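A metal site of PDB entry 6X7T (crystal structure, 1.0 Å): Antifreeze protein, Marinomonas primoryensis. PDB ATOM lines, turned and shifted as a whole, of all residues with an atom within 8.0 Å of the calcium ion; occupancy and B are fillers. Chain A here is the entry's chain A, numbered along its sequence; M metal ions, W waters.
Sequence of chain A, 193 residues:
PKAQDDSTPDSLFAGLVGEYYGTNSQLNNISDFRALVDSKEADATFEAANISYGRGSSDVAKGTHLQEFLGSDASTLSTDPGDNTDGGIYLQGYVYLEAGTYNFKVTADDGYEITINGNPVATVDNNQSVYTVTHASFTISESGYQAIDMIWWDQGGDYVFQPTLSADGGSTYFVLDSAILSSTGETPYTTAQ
The backbone NH (N) of Gly 63 lies within hydrogen-bond range of the side-chain carboxylate (OD1) of Asp 83 (2.8 Å). NE2 of Gln 67 lies close to OD1 of Asp 80.
The calcium ion is bound by O of Pro 81 (2.3 Å), water W1 (2.4 Å), water W3 (2.4 Å), water W2 (2.4 Å), O of Gly 63 (2.4 Å), water W4 (2.4 Å) and OD1 of Asp 80 (2.5 Å). The calcium ion has seven donor atoms within binding distance.
Within 4 Å of the calcium ion: Gly 63, Asp 80 and Pro 81. The nearest printed residue that does not touch the calcium ion is Gln 67 (4.4 Å).
Water W2 lies within hydrogen-bond range of O of Gly 82 (2.8 Å) and O of Ala 61 (3.1 Å).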
ATOM      1  N   TYR A  20      -9.593   6.104  -9.524  1.00  0.00           N
ATOM      2  CA  TYR A  20      -8.225   6.556  -9.297  1.00  0.00           C
ATOM      3  C   TYR A  20      -7.462   5.488  -8.523  1.00  0.00           C
ATOM      4  O   TYR A  20      -7.976   4.930  -7.539  1.00  0.00           O
ATOM      5  CB  TYR A  20      -8.224   7.881  -8.497  1.00  0.00           C
ATOM      6  CG  TYR A  20      -6.838   8.221  -8.013  1.00  0.00           C
ATOM      7  CD1 TYR A  20      -5.890   8.772  -8.873  1.00  0.00           C
ATOM      8  CD2 TYR A  20      -6.438   7.932  -6.718  1.00  0.00           C
ATOM      9  CE1 TYR A  20      -4.588   9.024  -8.446  1.00  0.00           C
ATOM     10  CE2 TYR A  20      -5.156   8.175  -6.285  1.00  0.00           C
ATOM     11  CZ  TYR A  20      -4.234   8.726  -7.159  1.00  0.00           C
ATOM     12  OH  TYR A  20      -2.932   8.966  -6.762  1.00  0.00           O
ATOM     13  N   VAL A  60       0.806  13.927  -9.287  1.00  0.00           N
ATOM     14  CA  VAL A  60      -0.656  13.916  -9.154  1.00  0.00           C
ATOM     15  C   VAL A  60      -1.078  13.204  -7.882  1.00  0.00           C
ATOM     16  O   VAL A  60      -2.150  13.487  -7.334  1.00  0.00           O
ATOM     17  CB  VAL A  60      -1.349  13.286 -10.384  1.00  0.00           C
ATOM     18  CG1 VAL A  60      -1.384  11.755 -10.300  1.00  0.00           C
ATOM     19  CG2 VAL A  60      -2.764  13.829 -10.533  1.00  0.00           C
ATOM     20  N   ALA A  61      -0.268  12.260  -7.414  1.00  0.00           N
ATOM     21  CA  ALA A  61      -0.667  11.358  -6.342  1.00  0.00           C
ATOM     22  C   ALA A  61      -0.366  11.892  -4.946  1.00  0.00           C
ATOM     23  O   ALA A  61      -0.654  11.199  -3.961  1.00  0.00           O
ATOM     24  CB  ALA A  61      -0.001   9.985  -6.565  1.00  0.00           C
ATOM     25  N   LYS A  62       0.189  13.112  -4.901  1.00  0.00           N
ATOM     26  CA  LYS A  62       0.562  13.712  -3.640  1.00  0.00           C
ATOM     27  C   LYS A  62      -0.460  14.778  -3.198  1.00  0.00           C
ATOM     28  O   LYS A  62      -1.035  15.475  -4.065  1.00  0.00           O
ATOM     29  CB  LYS A  62       1.950  14.332  -3.690  1.00  0.00           C
ATOM     30  CG  LYS A  62       3.055  13.297  -3.812  1.00  0.00           C
ATOM     31  CD  LYS A  62       3.273  12.489  -2.575  1.00  0.00           C
ATOM     32  CE  LYS A  62       4.412  11.506  -2.736  1.00  0.00           C
ATOM     33  NZ  LYS A  62       5.745  12.078  -2.387  1.00  0.00           N
ATOM     34  N   GLY A  63      -0.687  14.921  -1.870  1.00  0.00           N
ATOM     35  CA  GLY A  63      -1.461  16.037  -1.332  1.00  0.00           C
ATOM     36  C   GLY A  63      -2.830  16.142  -1.966  1.00  0.00           C
ATOM     37  O   GLY A  63      -3.553  15.147  -2.105  1.00  0.00           O
ATOM     38  N   THR A  64      -3.193  17.367  -2.334  1.00  0.00           N
ATOM     39  CA  THR A  64      -4.469  17.647  -2.971  1.00  0.00           C
ATOM     40  C   THR A  64      -4.333  17.811  -4.480  1.00  0.00           C
ATOM     41  O   THR A  64      -5.203  18.385  -5.135  1.00  0.00           O
ATOM     42  CB  THR A  64      -5.113  18.892  -2.353  1.00  0.00           C
ATOM     43  OG1 THR A  64      -4.261  20.037  -2.535  1.00  0.00           O
ATOM     44  CG2 THR A  64      -5.366  18.706  -0.853  1.00  0.00           C
ATOM     45  N   HIS A  65      -3.250  17.280  -5.057  1.00  0.00           N
ATOM     46  CA  HIS A  65      -3.028  17.463  -6.485  1.00  0.00           C
ATOM     47  C   HIS A  65      -4.080  16.767  -7.331  1.00  0.00           C
ATOM     48  O   HIS A  65      -4.447  17.283  -8.394  1.00  0.00           O
ATOM     49  CB  HIS A  65      -1.620  17.018  -6.855  1.00  0.00           C
ATOM     50  CG  HIS A  65      -0.572  17.853  -6.202  1.00  0.00           C
ATOM     51  ND1 HIS A  65       0.720  17.424  -6.012  1.00  0.00           N
ATOM     52  CD2 HIS A  65      -0.630  19.087  -5.663  1.00  0.00           C
ATOM     53  CE1 HIS A  65       1.423  18.358  -5.407  1.00  0.00           C
ATOM     54  NE2 HIS A  65       0.624  19.383  -5.170  1.00  0.00           N
ATOM     55  N   LEU A  66      -4.586  15.611  -6.887  1.00  0.00           N
ATOM     56  CA  LEU A  66      -5.630  14.949  -7.657  1.00  0.00           C
ATOM     57  C   LEU A  66      -6.883  15.799  -7.736  1.00  0.00           C
ATOM     58  O   LEU A  66      -7.518  15.907  -8.792  1.00  0.00           O
ATOM     59  CB  LEU A  66      -5.959  13.586  -7.050  1.00  0.00           C
ATOM     60  CG  LEU A  66      -7.085  12.805  -7.747  1.00  0.00           C
ATOM     61  CD1 LEU A  66      -6.688  12.398  -9.151  1.00  0.00           C
ATOM     62  CD2 LEU A  66      -7.472  11.613  -6.886  1.00  0.00           C
ATOM     63  N   GLN A  67      -7.270  16.408  -6.602  1.00  0.00           N
ATOM     64  CA  GLN A  67      -8.430  17.282  -6.572  1.00  0.00           C
ATOM     65  C   GLN A  67      -8.256  18.441  -7.553  1.00  0.00           C
ATOM     66  O   GLN A  67      -9.185  18.813  -8.282  1.00  0.00           O
ATOM     67  CB  GLN A  67      -8.606  17.850  -5.169  1.00  0.00           C
ATOM     68  CG  GLN A  67      -9.172  16.882  -4.148  1.00  0.00           C
ATOM     69  CD  GLN A  67      -8.191  15.894  -3.537  1.00  0.00           C
ATOM     70  OE1 GLN A  67      -7.006  15.804  -3.896  1.00  0.00           O
ATOM     71  NE2 GLN A  67      -8.691  15.124  -2.579  1.00  0.00           N
ATOM     72  N   LEU A  77     -15.580  12.883  -5.736  1.00  0.00           N
ATOM     73  CA  LEU A  77     -14.659  11.891  -5.183  1.00  0.00           C
ATOM     74  C   LEU A  77     -15.278  11.162  -3.994  1.00  0.00           C
ATOM     75  O   LEU A  77     -15.879  11.771  -3.100  1.00  0.00           O
ATOM     76  CB  LEU A  77     -13.361  12.568  -4.718  1.00  0.00           C
ATOM     77  CG  LEU A  77     -12.328  12.862  -5.803  1.00  0.00           C
ATOM     78  CD1 LEU A  77     -11.292  13.838  -5.309  1.00  0.00           C
ATOM     79  CD2 LEU A  77     -11.651  11.589  -6.257  1.00  0.00           C
ATOM     80  N   THR A  79     -13.526   9.606  -1.699  1.00  0.00           N
ATOM     81  CA  THR A  79     -12.622   9.780  -0.573  1.00  0.00           C
ATOM     82  C   THR A  79     -11.465  10.626  -1.089  1.00  0.00           C
ATOM     83  O   THR A  79     -11.305  10.814  -2.305  1.00  0.00           O
ATOM     84  CB  THR A  79     -12.156   8.404  -0.066  1.00  0.00           C
ATOM     85  OG1 THR A  79     -11.493   8.540   1.189  1.00  0.00           O
ATOM     86  CG2 THR A  79     -11.226   7.764  -1.067  1.00  0.00           C
ATOM     87  N   ASP A  80     -10.672  11.165  -0.161  1.00  0.00           N
ATOM     88  CA  ASP A  80      -9.432  11.860  -0.470  1.00  0.00           C
ATOM     89  C   ASP A  80      -8.297  10.857  -0.303  1.00  0.00           C
ATOM     90  O   ASP A  80      -7.962  10.505   0.831  1.00  0.00           O
ATOM     91  CB  ASP A  80      -9.249  13.036   0.490  1.00  0.00           C
ATOM     92  CG  ASP A  80      -7.949  13.775   0.314  1.00  0.00           C
ATOM     93  OD1 ASP A  80      -7.187  13.454  -0.631  1.00  0.00           O
ATOM     94  OD2 ASP A  80      -7.707  14.700   1.119  1.00  0.00           O
ATOM     95  N   PRO A  81      -7.717  10.347  -1.388  1.00  0.00           N
ATOM     96  CA  PRO A  81      -6.658   9.348  -1.254  1.00  0.00           C
ATOM     97  C   PRO A  81      -5.466   9.906  -0.480  1.00  0.00           C
ATOM     98  O   PRO A  81      -5.194  11.109  -0.509  1.00  0.00           O
ATOM     99  CB  PRO A  81      -6.247   9.032  -2.699  1.00  0.00           C
ATOM    100  CG  PRO A  81      -7.224   9.679  -3.573  1.00  0.00           C
ATOM    101  CD  PRO A  81      -7.945  10.730  -2.794  1.00  0.00           C
ATOM    102  N   GLY A  82      -4.743   9.018   0.187  1.00  0.00           N
ATOM    103  CA  GLY A  82      -3.472   9.374   0.769  1.00  0.00           C
ATOM    104  C   GLY A  82      -2.400   9.534  -0.289  1.00  0.00           C
ATOM    105  O   GLY A  82      -2.629   9.417  -1.488  1.00  0.00           O
ATOM    106  N   ASP A  83      -1.171   9.851   0.175  1.00  0.00           N
ATOM    107  CA  ASP A  83      -0.075  10.106  -0.750  1.00  0.00           C
ATOM    108  C   ASP A  83       0.440   8.809  -1.379  1.00  0.00           C
ATOM    109  O   ASP A  83       0.491   7.748  -0.745  1.00  0.00           O
ATOM    110  CB  ASP A  83       1.108  10.723  -0.006  1.00  0.00           C
ATOM    111  CG  ASP A  83       0.954  12.193   0.324  1.00  0.00           C
ATOM    112  OD1 ASP A  83      -0.063  12.820  -0.085  1.00  0.00           O
ATOM    113  OD2 ASP A  83       1.902  12.716   0.946  1.00  0.00           O
ATOM    114  N   ASN A  84       0.844   8.941  -2.624  1.00  0.00           N
ATOM    115  CA  ASN A  84       1.597   7.909  -3.361  1.00  0.00           C
ATOM    116  C   ASN A  84       2.568   8.666  -4.275  1.00  0.00           C
ATOM    117  O   ASN A  84       2.416   9.884  -4.496  1.00  0.00           O
ATOM    118  CB  ASN A  84       0.686   7.015  -4.194  1.00  0.00           C
ATOM    119  CG  ASN A  84       0.048   5.869  -3.416  1.00  0.00           C
ATOM    120  OD1 ASN A  84       0.759   4.971  -2.911  1.00  0.00           O
ATOM    121  ND2 ASN A  84      -1.261   5.888  -3.357  1.00  0.00           N
HETATM  122 CA    CA M   1      -4.745  13.322  -1.042  1.00  0.00          CA
HETATM  123  O   HOH W   1      -5.090  15.119   0.489  1.00  0.00           O
HETATM  124  O   HOH W   2      -3.267  12.017  -2.452  1.00  0.00           O
HETATM  125  O   HOH W   3      -2.837  13.069   0.386  1.00  0.00           O
HETATM  126  O   HOH W   4      -5.655  13.455  -3.312  1.00  0.00           O
